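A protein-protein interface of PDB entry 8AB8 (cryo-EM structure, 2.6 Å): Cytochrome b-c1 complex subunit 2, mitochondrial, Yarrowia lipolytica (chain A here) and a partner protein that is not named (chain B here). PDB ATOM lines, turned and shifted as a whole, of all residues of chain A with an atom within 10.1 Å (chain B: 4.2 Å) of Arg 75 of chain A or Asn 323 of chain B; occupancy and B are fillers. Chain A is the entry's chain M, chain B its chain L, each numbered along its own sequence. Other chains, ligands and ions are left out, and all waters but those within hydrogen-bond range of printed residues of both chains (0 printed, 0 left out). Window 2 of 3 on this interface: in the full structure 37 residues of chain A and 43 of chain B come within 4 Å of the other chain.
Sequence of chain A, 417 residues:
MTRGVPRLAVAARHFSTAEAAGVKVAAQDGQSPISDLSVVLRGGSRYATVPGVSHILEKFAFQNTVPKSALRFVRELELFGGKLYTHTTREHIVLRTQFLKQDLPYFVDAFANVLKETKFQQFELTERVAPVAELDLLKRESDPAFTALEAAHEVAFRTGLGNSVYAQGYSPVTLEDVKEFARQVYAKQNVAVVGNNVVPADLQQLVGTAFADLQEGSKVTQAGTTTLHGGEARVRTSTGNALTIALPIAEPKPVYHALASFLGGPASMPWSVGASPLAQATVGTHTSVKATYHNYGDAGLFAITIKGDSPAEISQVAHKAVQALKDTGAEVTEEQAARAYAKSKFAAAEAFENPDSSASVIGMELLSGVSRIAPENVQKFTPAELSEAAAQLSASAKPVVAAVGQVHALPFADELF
The backbone carbonyl oxygen (O) of His 316 of chain B lies within hydrogen-bond range of the guanidinium group (NE) of Arg 75 of chain A.
N of Gly 318 of chain B is in hydrogen-bond range of OE2 of Glu 78 of chain A, 3.3 Å away.
Of the 12 printed residues of chain B, 4 touch a printed residue of chain A.
Printed residues of chain B that touch a printed residue of chain A: His 316, Gln 317, Gly 318 and Asn 323.
Hydrophobic or aromatic side chains of chain B within 4 Å of the printed part of chain A: His 316.
Of the 19 printed residues of chain A, 5 touch a printed residue of chain B.
Hydrophobic or aromatic side chains of chain A that line the printed part of chain B: Ala 70, Leu 71 and Val 74.
Among the printed residues, 9 pairs touch across the chains.
Among the printed residues, no Asp or Glu carboxylate lies within 4 Å of a Lys or Arg side-chain nitrogen of the other chain.
Arg 75 of chain A touches just these residues of chain B: His 316 (2.7 Å), Gln 317 (3.6 Å), Gly 318 (3.5 Å) and Asn 323 (3.95 Å).
Printed residues of chain A within 4 Å of Asn 323 of chain B: Arg 75.
Printed residues of chain A within 4 Å of Gly 318 of chain B: Arg 75 (3.5 Å) and Glu 78 (3.3 Å).
No residue of chain A comes within 4 Å of Ser 322 of chain B.
No residue of chain A comes within 4 Å of Glu 327 of chain B.
Printed residues of chain B within 4 Å of Ala 70 of chain A: His 316 (3.8 Å).
Printed residues of chain A within 4 Å of His 316 of chain B: Ala 70 (3.8 Å), Leu 71 (3.8 Å), Val 74 (3.6 Å) and Arg 75 (2.7 Å).
Of the printed residues of chain B, Leu 71 of chain A touches His 316.
Of the printed residues of chain B, Val 74 of chain A touches His 316.
Tyr 106 of chain A touches none of the printed residues of chain B.
The nearest printed residue of chain B that does not touch Arg 75 of chain A is Ser 319 of chain B (5.8 Å).
The nearest printed residue of chain B that does not touch Leu 71 of chain A is Gln 317 of chain B (5.9 Å).
NE2 of Gln 317 of chain B sits at hydrogen-bond distance from OG of Ser 322 of chain B (3.0 Å).
O of Gln 317 of chain B lies within hydrogen-bond range of ND2 of Asn 323 of chain B.
O of Ser 319 of chain B sits at hydrogen-bond distance from ND2 of Asn 323 of chain B, 2.8 Å away.
OG of Ser 326 of chain B lies within hydrogen-bond range of O of Asn 323 of chain B, 3.3 Å away.
NE2 of His 316 of chain B touches CB of Ala 70 of chain A, 3.8 Å away.
His 316 of chain B touches Leu 71 of chain A (ND1 to CB, 3.8 Å).
Val 74 of chain A touches His 316 of chain B.
Arg 75 of chain A touches Gln 317 of chain B.
Arg 75 of chain A touches Gly 318 of chain B.
Arg 75 of chain A touches Asn 323 of chain B.
Glu 78 of chain A touches Gln 317 of chain B (OE1 to CA, 3.5 Å).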
ATOM      1  N   PHE A  62     -21.998  10.195 -11.070  1.00  0.00           N
ATOM      2  CA  PHE A  62     -22.592   9.413 -12.142  1.00  0.00           C
ATOM      3  C   PHE A  62     -21.845   9.605 -13.465  1.00  0.00           C
ATOM      4  O   PHE A  62     -22.438   9.478 -14.531  1.00  0.00           O
ATOM      5  CB  PHE A  62     -24.100   9.653 -12.201  1.00  0.00           C
ATOM      6  CG  PHE A  62     -24.806   9.267 -10.927  1.00  0.00           C
ATOM      7  CD1 PHE A  62     -25.120   7.940 -10.675  1.00  0.00           C
ATOM      8  CD2 PHE A  62     -25.135  10.217  -9.966  1.00  0.00           C
ATOM      9  CE1 PHE A  62     -25.769   7.571  -9.504  1.00  0.00           C
ATOM     10  CE2 PHE A  62     -25.756   9.843  -8.781  1.00  0.00           C
ATOM     11  CZ  PHE A  62     -26.093   8.523  -8.562  1.00  0.00           C
ATOM     12  N   LYS A  68     -19.741   0.355 -13.973  1.00  0.00           N
ATOM     13  CA  LYS A  68     -20.806   0.820 -14.849  1.00  0.00           C
ATOM     14  C   LYS A  68     -20.449   2.182 -15.433  1.00  0.00           C
ATOM     15  O   LYS A  68     -20.153   3.110 -14.689  1.00  0.00           O
ATOM     16  CB  LYS A  68     -22.138   0.835 -14.088  1.00  0.00           C
ATOM     17  CG  LYS A  68     -23.381   1.088 -14.932  1.00  0.00           C
ATOM     18  CD  LYS A  68     -24.641   1.345 -14.115  1.00  0.00           C
ATOM     19  CE  LYS A  68     -25.164   0.168 -13.308  1.00  0.00           C
ATOM     20  NZ  LYS A  68     -25.232  -1.088 -14.095  1.00  0.00           N
ATOM     21  N   SER A  69     -20.486   2.294 -16.764  1.00  0.00           N
ATOM     22  CA  SER A  69     -20.144   3.541 -17.430  1.00  0.00           C
ATOM     23  C   SER A  69     -21.273   4.555 -17.275  1.00  0.00           C
ATOM     24  O   SER A  69     -22.422   4.179 -17.046  1.00  0.00           O
ATOM     25  CB  SER A  69     -19.852   3.284 -18.871  1.00  0.00           C
ATOM     26  OG  SER A  69     -21.048   3.015 -19.589  1.00  0.00           O
ATOM     27  N   ALA A  70     -20.946   5.841 -17.430  1.00  0.00           N
ATOM     28  CA  ALA A  70     -21.957   6.890 -17.396  1.00  0.00           C
ATOM     29  C   ALA A  70     -23.047   6.604 -18.427  1.00  0.00           C
ATOM     30  O   ALA A  70     -24.234   6.767 -18.148  1.00  0.00           O
ATOM     31  CB  ALA A  70     -21.308   8.229 -17.629  1.00  0.00           C
ATOM     32  N   LEU A  71     -22.622   6.144 -19.607  1.00  0.00           N
ATOM     33  CA  LEU A  71     -23.540   5.852 -20.687  1.00  0.00           C
ATOM     34  C   LEU A  71     -24.458   4.711 -20.268  1.00  0.00           C
ATOM     35  O   LEU A  71     -25.673   4.820 -20.405  1.00  0.00           O
ATOM     36  CB  LEU A  71     -22.739   5.507 -21.943  1.00  0.00           C
ATOM     37  CG  LEU A  71     -23.494   4.752 -23.038  1.00  0.00           C
ATOM     38  CD1 LEU A  71     -24.565   5.617 -23.696  1.00  0.00           C
ATOM     39  CD2 LEU A  71     -22.515   4.267 -24.088  1.00  0.00           C
ATOM     40  N   ARG A  72     -23.884   3.637 -19.728  1.00  0.00           N
ATOM     41  CA  ARG A  72     -24.756   2.538 -19.365  1.00  0.00           C
ATOM     42  C   ARG A  72     -25.733   2.947 -18.257  1.00  0.00           C
ATOM     43  O   ARG A  72     -26.867   2.478 -18.224  1.00  0.00           O
ATOM     44  CB  ARG A  72     -23.978   1.299 -18.952  1.00  0.00           C
ATOM     45  CG  ARG A  72     -24.953   0.193 -18.591  1.00  0.00           C
ATOM     46  CD  ARG A  72     -24.512  -1.241 -18.740  1.00  0.00           C
ATOM     47  NE  ARG A  72     -23.845  -1.597 -19.983  1.00  0.00           N
ATOM     48  CZ  ARG A  72     -24.305  -2.456 -20.889  1.00  0.00           C
ATOM     49  NH1 ARG A  72     -25.468  -3.066 -20.721  1.00  0.00           N
ATOM     50  NH2 ARG A  72     -23.588  -2.704 -21.971  1.00  0.00           N
ATOM     51  N   PHE A  73     -25.273   3.785 -17.330  1.00  0.00           N
ATOM     52  CA  PHE A  73     -26.136   4.224 -16.253  1.00  0.00           C
ATOM     53  C   PHE A  73     -27.334   4.998 -16.798  1.00  0.00           C
ATOM     54  O   PHE A  73     -28.467   4.725 -16.417  1.00  0.00           O
ATOM     55  CB  PHE A  73     -25.360   5.045 -15.224  1.00  0.00           C
ATOM     56  CG  PHE A  73     -26.253   5.607 -14.153  1.00  0.00           C
ATOM     57  CD1 PHE A  73     -26.852   4.768 -13.218  1.00  0.00           C
ATOM     58  CD2 PHE A  73     -26.538   6.966 -14.103  1.00  0.00           C
ATOM     59  CE1 PHE A  73     -27.696   5.278 -12.238  1.00  0.00           C
ATOM     60  CE2 PHE A  73     -27.380   7.479 -13.121  1.00  0.00           C
ATOM     61  CZ  PHE A  73     -27.959   6.634 -12.190  1.00  0.00           C
ATOM     62  N   VAL A  74     -27.080   5.968 -17.673  1.00  0.00           N
ATOM     63  CA  VAL A  74     -28.162   6.784 -18.191  1.00  0.00           C
ATOM     64  C   VAL A  74     -29.148   5.918 -18.973  1.00  0.00           C
ATOM     65  O   VAL A  74     -30.347   6.137 -18.869  1.00  0.00           O
ATOM     66  CB  VAL A  74     -27.632   7.944 -19.051  1.00  0.00           C
ATOM     67  CG1 VAL A  74     -28.750   8.646 -19.815  1.00  0.00           C
ATOM     68  CG2 VAL A  74     -26.837   8.935 -18.223  1.00  0.00           C
ATOM     69  N   ARG A  75     -28.656   4.957 -19.764  1.00  0.00           N
ATOM     70  CA  ARG A  75     -29.556   4.137 -20.561  1.00  0.00           C
ATOM     71  C   ARG A  75     -30.432   3.271 -19.657  1.00  0.00           C
ATOM     72  O   ARG A  75     -31.591   3.010 -19.972  1.00  0.00           O
ATOM     73  CB  ARG A  75     -28.805   3.278 -21.581  1.00  0.00           C
ATOM     74  CG  ARG A  75     -28.106   4.067 -22.681  1.00  0.00           C
ATOM     75  CD  ARG A  75     -28.981   4.998 -23.496  1.00  0.00           C
ATOM     76  NE  ARG A  75     -28.181   5.613 -24.543  1.00  0.00           N
ATOM     77  CZ  ARG A  75     -27.995   5.103 -25.759  1.00  0.00           C
ATOM     78  NH1 ARG A  75     -28.573   3.964 -26.097  1.00  0.00           N
ATOM     79  NH2 ARG A  75     -27.233   5.737 -26.636  1.00  0.00           N
ATOM     80  N   GLU A  76     -29.885   2.844 -18.518  1.00  0.00           N
ATOM     81  CA  GLU A  76     -30.638   1.955 -17.650  1.00  0.00           C
ATOM     82  C   GLU A  76     -31.599   2.750 -16.776  1.00  0.00           C
ATOM     83  O   GLU A  76     -32.687   2.272 -16.456  1.00  0.00           O
ATOM     84  CB  GLU A  76     -29.699   1.136 -16.785  1.00  0.00           C
ATOM     85  CG  GLU A  76     -29.027   0.027 -17.553  1.00  0.00           C
ATOM     86  CD  GLU A  76     -28.039  -0.757 -16.708  1.00  0.00           C
ATOM     87  OE1 GLU A  76     -27.664  -1.875 -17.110  1.00  0.00           O
ATOM     88  OE2 GLU A  76     -27.648  -0.248 -15.638  1.00  0.00           O
ATOM     89  N   LEU A  77     -31.179   3.957 -16.388  1.00  0.00           N
ATOM     90  CA  LEU A  77     -32.019   4.860 -15.625  1.00  0.00           C
ATOM     91  C   LEU A  77     -33.272   5.215 -16.430  1.00  0.00           C
ATOM     92  O   LEU A  77     -34.336   5.383 -15.845  1.00  0.00           O
ATOM     93  CB  LEU A  77     -31.173   6.083 -15.261  1.00  0.00           C
ATOM     94  CG  LEU A  77     -31.878   7.277 -14.624  1.00  0.00           C
ATOM     95  CD1 LEU A  77     -31.914   7.138 -13.115  1.00  0.00           C
ATOM     96  CD2 LEU A  77     -31.160   8.562 -15.002  1.00  0.00           C
ATOM     97  N   GLU A  78     -33.157   5.293 -17.767  1.00  0.00           N
ATOM     98  CA  GLU A  78     -34.302   5.600 -18.618  1.00  0.00           C
ATOM     99  C   GLU A  78     -35.260   4.414 -18.681  1.00  0.00           C
ATOM    100  O   GLU A  78     -36.464   4.626 -18.837  1.00  0.00           O
ATOM    101  CB  GLU A  78     -33.916   5.962 -20.058  1.00  0.00           C
ATOM    102  CG  GLU A  78     -33.167   7.275 -20.229  1.00  0.00           C
ATOM    103  CD  GLU A  78     -32.537   7.483 -21.608  1.00  0.00           C
ATOM    104  OE1 GLU A  78     -32.830   8.511 -22.278  1.00  0.00           O
ATOM    105  OE2 GLU A  78     -31.714   6.632 -21.995  1.00  0.00           O
ATOM    106  N   LEU A  79     -34.736   3.186 -18.555  1.00  0.00           N
ATOM    107  CA  LEU A  79     -35.581   2.000 -18.519  1.00  0.00           C
ATOM    108  C   LEU A  79     -36.387   1.894 -17.226  1.00  0.00           C
ATOM    109  O   LEU A  79     -37.403   1.197 -17.191  1.00  0.00           O
ATOM    110  CB  LEU A  79     -34.713   0.753 -18.665  1.00  0.00           C
ATOM    111  CG  LEU A  79     -34.068   0.580 -20.028  1.00  0.00           C
ATOM    112  CD1 LEU A  79     -33.232  -0.684 -20.061  1.00  0.00           C
ATOM    113  CD2 LEU A  79     -35.108   0.564 -21.135  1.00  0.00           C
ATOM    114  N   PHE A  80     -35.909   2.531 -16.151  1.00  0.00           N
ATOM    115  CA  PHE A  80     -36.641   2.588 -14.898  1.00  0.00           C
ATOM    116  C   PHE A  80     -37.487   3.857 -14.849  1.00  0.00           C
ATOM    117  O   PHE A  80     -38.284   4.050 -13.933  1.00  0.00           O
ATOM    118  CB  PHE A  80     -35.653   2.636 -13.734  1.00  0.00           C
ATOM    119  CG  PHE A  80     -35.099   1.313 -13.281  1.00  0.00           C
ATOM    120  CD1 PHE A  80     -35.948   0.266 -12.959  1.00  0.00           C
ATOM    121  CD2 PHE A  80     -33.729   1.114 -13.159  1.00  0.00           C
ATOM    122  CE1 PHE A  80     -35.454  -0.938 -12.481  1.00  0.00           C
ATOM    123  CE2 PHE A  80     -33.228  -0.107 -12.726  1.00  0.00           C
ATOM    124  CZ  PHE A  80     -34.092  -1.131 -12.387  1.00  0.00           C
ATOM    125  N   GLY A  81     -37.257   4.748 -15.812  1.00  0.00           N
ATOM    126  CA  GLY A  81     -37.857   6.068 -15.814  1.00  0.00           C
ATOM    127  C   GLY A  81     -37.438   6.914 -14.614  1.00  0.00           C
ATOM    128  O   GLY A  81     -38.148   7.845 -14.246  1.00  0.00           O
ATOM    129  N   GLY A  82     -36.291   6.596 -14.002  1.00  0.00           N
ATOM    130  CA  GLY A  82     -35.789   7.385 -12.886  1.00  0.00           C
ATOM    131  C   GLY A  82     -35.255   8.745 -13.334  1.00  0.00           C
ATOM    132  O   GLY A  82     -35.013   8.967 -14.518  1.00  0.00           O
ATOM    133  N   LEU A  84     -32.417  12.042 -12.037  1.00  0.00           N
ATOM    134  CA  LEU A  84     -31.236  12.311 -11.246  1.00  0.00           C
ATOM    135  C   LEU A  84     -31.126  13.811 -11.009  1.00  0.00           C
ATOM    136  O   LEU A  84     -31.279  14.579 -11.944  1.00  0.00           O
ATOM    137  CB  LEU A  84     -30.064  11.792 -12.073  1.00  0.00           C
ATOM    138  CG  LEU A  84     -28.691  12.004 -11.462  1.00  0.00           C
ATOM    139  CD1 LEU A  84     -28.559  11.236 -10.156  1.00  0.00           C
ATOM    140  CD2 LEU A  84     -27.635  11.582 -12.459  1.00  0.00           C
ATOM    141  N   TYR A 106     -31.515  -1.087  -7.075  1.00  0.00           N
ATOM    142  CA  TYR A 106     -30.693  -0.558  -8.148  1.00  0.00           C
ATOM    143  C   TYR A 106     -30.072   0.782  -7.747  1.00  0.00           C
ATOM    144  O   TYR A 106     -28.888   1.011  -7.981  1.00  0.00           O
ATOM    145  CB  TYR A 106     -31.501  -0.455  -9.441  1.00  0.00           C
ATOM    146  CG  TYR A 106     -30.703   0.100 -10.588  1.00  0.00           C
ATOM    147  CD1 TYR A 106     -30.657   1.464 -10.831  1.00  0.00           C
ATOM    148  CD2 TYR A 106     -29.966  -0.745 -11.406  1.00  0.00           C
ATOM    149  CE1 TYR A 106     -29.896   1.976 -11.870  1.00  0.00           C
ATOM    150  CE2 TYR A 106     -29.210  -0.253 -12.457  1.00  0.00           C
ATOM    151  CZ  TYR A 106     -29.182   1.111 -12.691  1.00  0.00           C
ATOM    152  OH  TYR A 106     -28.420   1.572 -13.722  1.00  0.00           O
ATOM    153  N   PHE A 107     -30.879   1.680  -7.172  1.00  0.00           N
ATOM    154  CA  PHE A 107     -30.428   3.028  -6.858  1.00  0.00           C
ATOM    155  C   PHE A 107     -29.427   3.046  -5.713  1.00  0.00           C
ATOM    156  O   PHE A 107     -28.527   3.883  -5.704  1.00  0.00           O
ATOM    157  CB  PHE A 107     -31.618   3.980  -6.714  1.00  0.00           C
ATOM    158  CG  PHE A 107     -32.241   4.165  -8.066  1.00  0.00           C
ATOM    159  CD1 PHE A 107     -31.684   5.051  -8.979  1.00  0.00           C
ATOM    160  CD2 PHE A 107     -33.281   3.341  -8.475  1.00  0.00           C
ATOM    161  CE1 PHE A 107     -32.213   5.163 -10.255  1.00  0.00           C
ATOM    162  CE2 PHE A 107     -33.803   3.448  -9.754  1.00  0.00           C
ATOM    163  CZ  PHE A 107     -33.270   4.363 -10.639  1.00  0.00           C
ATOM    164  N   HIS B 316     -26.057  11.142 -23.147  1.00  0.00           N
ATOM    165  CA  HIS B 316     -26.115   9.693 -23.117  1.00  0.00           C
ATOM    166  C   HIS B 316     -27.518   9.147 -23.355  1.00  0.00           C
ATOM    167  O   HIS B 316     -27.733   7.946 -23.215  1.00  0.00           O
ATOM    168  CB  HIS B 316     -25.598   9.181 -21.782  1.00  0.00           C
ATOM    169  CG  HIS B 316     -24.175   9.519 -21.521  1.00  0.00           C
ATOM    170  ND1 HIS B 316     -23.164   9.213 -22.414  1.00  0.00           N
ATOM    171  CD2 HIS B 316     -23.588  10.118 -20.463  1.00  0.00           C
ATOM    172  CE1 HIS B 316     -22.012   9.622 -21.922  1.00  0.00           C
ATOM    173  NE2 HIS B 316     -22.243  10.171 -20.717  1.00  0.00           N
ATOM    174  N   GLN B 317     -28.469  10.007 -23.714  1.00  0.00           N
ATOM    175  CA  GLN B 317     -29.849   9.568 -23.864  1.00  0.00           C
ATOM    176  C   GLN B 317     -29.991   8.625 -25.056  1.00  0.00           C
ATOM    177  O   GLN B 317     -29.245   8.719 -26.027  1.00  0.00           O
ATOM    178  CB  GLN B 317     -30.759  10.768 -24.078  1.00  0.00           C
ATOM    179  CG  GLN B 317     -30.892  11.637 -22.846  1.00  0.00           C
ATOM    180  CD  GLN B 317     -31.826  12.795 -23.076  1.00  0.00           C
ATOM    181  OE1 GLN B 317     -32.685  13.088 -22.250  1.00  0.00           O
ATOM    182  NE2 GLN B 317     -31.659  13.475 -24.199  1.00  0.00           N
ATOM    183  N   GLY B 318     -30.987   7.738 -24.984  1.00  0.00           N
ATOM    184  CA  GLY B 318     -31.179   6.689 -25.972  1.00  0.00           C
ATOM    185  C   GLY B 318     -31.811   7.159 -27.283  1.00  0.00           C
ATOM    186  O   GLY B 318     -31.614   6.524 -28.320  1.00  0.00           O
ATOM    187  N   SER B 319     -32.585   8.250 -27.229  1.00  0.00           N
ATOM    188  CA  SER B 319     -33.256   8.825 -28.388  1.00  0.00           C
ATOM    189  C   SER B 319     -32.267   9.074 -29.526  1.00  0.00           C
ATOM    190  O   SER B 319     -31.252   9.726 -29.319  1.00  0.00           O
ATOM    191  CB  SER B 319     -33.934  10.110 -27.990  1.00  0.00           C
ATOM    192  OG  SER B 319     -34.288  10.892 -29.126  1.00  0.00           O
ATOM    193  N   ARG B 320     -32.602   8.603 -30.732  1.00  0.00           N
ATOM    194  CA  ARG B 320     -31.789   8.824 -31.916  1.00  0.00           C
ATOM    195  C   ARG B 320     -31.575  10.315 -32.207  1.00  0.00           C
ATOM    196  O   ARG B 320     -30.457  10.728 -32.532  1.00  0.00           O
ATOM    197  CB  ARG B 320     -32.374   8.071 -33.113  1.00  0.00           C
ATOM    198  CG  ARG B 320     -31.651   8.341 -34.424  1.00  0.00           C
ATOM    199  CD  ARG B 320     -30.210   7.870 -34.331  1.00  0.00           C
ATOM    200  NE  ARG B 320     -29.449   8.006 -35.564  1.00  0.00           N
ATOM    201  CZ  ARG B 320     -28.118   8.004 -35.645  1.00  0.00           C
ATOM    202  NH1 ARG B 320     -27.378   7.905 -34.553  1.00  0.00           N
ATOM    203  NH2 ARG B 320     -27.534   8.132 -36.823  1.00  0.00           N
ATOM    204  N   LEU B 321     -32.643  11.118 -32.098  1.00  0.00           N
ATOM    205  CA  LEU B 321     -32.515  12.539 -32.384  1.00  0.00           C
ATOM    206  C   LEU B 321     -31.541  13.185 -31.406  1.00  0.00           C
ATOM    207  O   LEU B 321     -30.718  14.010 -31.800  1.00  0.00           O
ATOM    208  CB  LEU B 321     -33.871  13.254 -32.369  1.00  0.00           C
ATOM    209  CG  LEU B 321     -33.784  14.744 -32.718  1.00  0.00           C
ATOM    210  CD1 LEU B 321     -33.212  14.963 -34.116  1.00  0.00           C
ATOM    211  CD2 LEU B 321     -35.114  15.458 -32.555  1.00  0.00           C
ATOM    212  N   SER B 322     -31.631  12.776 -30.141  1.00  0.00           N
ATOM    213  CA  SER B 322     -30.739  13.266 -29.110  1.00  0.00           C
ATOM    214  C   SER B 322     -29.291  13.011 -29.515  1.00  0.00           C
ATOM    215  O   SER B 322     -28.467  13.917 -29.435  1.00  0.00           O
ATOM    216  CB  SER B 322     -31.063  12.630 -27.798  1.00  0.00           C
ATOM    217  OG  SER B 322     -30.181  13.098 -26.791  1.00  0.00           O
ATOM    218  N   ASN B 323     -29.005  11.786 -29.970  1.00  0.00           N
ATOM    219  CA  ASN B 323     -27.662  11.408 -30.368  1.00  0.00           C
ATOM    220  C   ASN B 323     -27.183  12.253 -31.541  1.00  0.00           C
ATOM    221  O   ASN B 323     -26.081  12.780 -31.491  1.00  0.00           O
ATOM    222  CB  ASN B 323     -27.562   9.911 -30.631  1.00  0.00           C
ATOM    223  CG  ASN B 323     -27.617   9.134 -29.335  1.00  0.00           C
ATOM    224  OD1 ASN B 323     -26.649   9.130 -28.579  1.00  0.00           O
ATOM    225  ND2 ASN B 323     -28.741   8.500 -29.050  1.00  0.00           N
ATOM    226  N   ILE B 324     -28.021  12.420 -32.570  1.00  0.00           N
ATOM    227  CA  ILE B 324     -27.621  13.192 -33.740  1.00  0.00           C
ATOM    228  C   ILE B 324     -27.290  14.628 -33.335  1.00  0.00           C
ATOM    229  O   ILE B 324     -26.276  15.182 -33.766  1.00  0.00           O
ATOM    230  CB  ILE B 324     -28.693  13.145 -34.852  1.00  0.00           C
ATOM    231  CG1 ILE B 324     -28.827  11.741 -35.443  1.00  0.00           C
ATOM    232  CG2 ILE B 324     -28.415  14.191 -35.933  1.00  0.00           C
ATOM    233  CD1 ILE B 324     -30.173  11.475 -36.074  1.00  0.00           C
ATOM    234  N   VAL B 325     -28.181  15.225 -32.544  1.00  0.00           N
ATOM    235  CA  VAL B 325     -28.077  16.624 -32.178  1.00  0.00           C
ATOM    236  C   VAL B 325     -26.858  16.838 -31.286  1.00  0.00           C
ATOM    237  O   VAL B 325     -26.119  17.791 -31.502  1.00  0.00           O
ATOM    238  CB  VAL B 325     -29.382  17.120 -31.534  1.00  0.00           C
ATOM    239  CG1 VAL B 325     -29.197  18.422 -30.766  1.00  0.00           C
ATOM    240  CG2 VAL B 325     -30.470  17.253 -32.587  1.00  0.00           C
ATOM    241  N   SER B 326     -26.638  15.949 -30.312  1.00  0.00           N
ATOM    242  CA  SER B 326     -25.528  16.154 -29.395  1.00  0.00           C
ATOM    243  C   SER B 326     -24.186  15.962 -30.096  1.00  0.00           C
ATOM    244  O   SER B 326     -23.309  16.798 -29.928  1.00  0.00           O
ATOM    245  CB  SER B 326     -25.641  15.357 -28.132  1.00  0.00           C
ATOM    246  OG  SER B 326     -25.640  13.974 -28.429  1.00  0.00           O
ATOM    247  N   GLU B 327     -24.050  14.908 -30.911  1.00  0.00           N
ATOM    248  CA  GLU B 327     -22.787  14.622 -31.585  1.00  0.00           C
ATOM    249  C   GLU B 327     -22.389  15.745 -32.548  1.00  0.00           C
ATOM    250  O   GLU B 327     -21.206  16.007 -32.754  1.00  0.00           O
ATOM    251  CB  GLU B 327     -22.858  13.289 -32.331  1.00  0.00           C
ATOM    252  CG  GLU B 327     -22.887  12.086 -31.408  1.00  0.00           C
ATOM    253  CD  GLU B 327     -23.117  10.750 -32.096  1.00  0.00           C
ATOM    254  OE1 GLU B 327     -24.186  10.575 -32.726  1.00  0.00           O
ATOM    255  OE2 GLU B 327     -22.223   9.885 -32.007  1.00  0.00           O
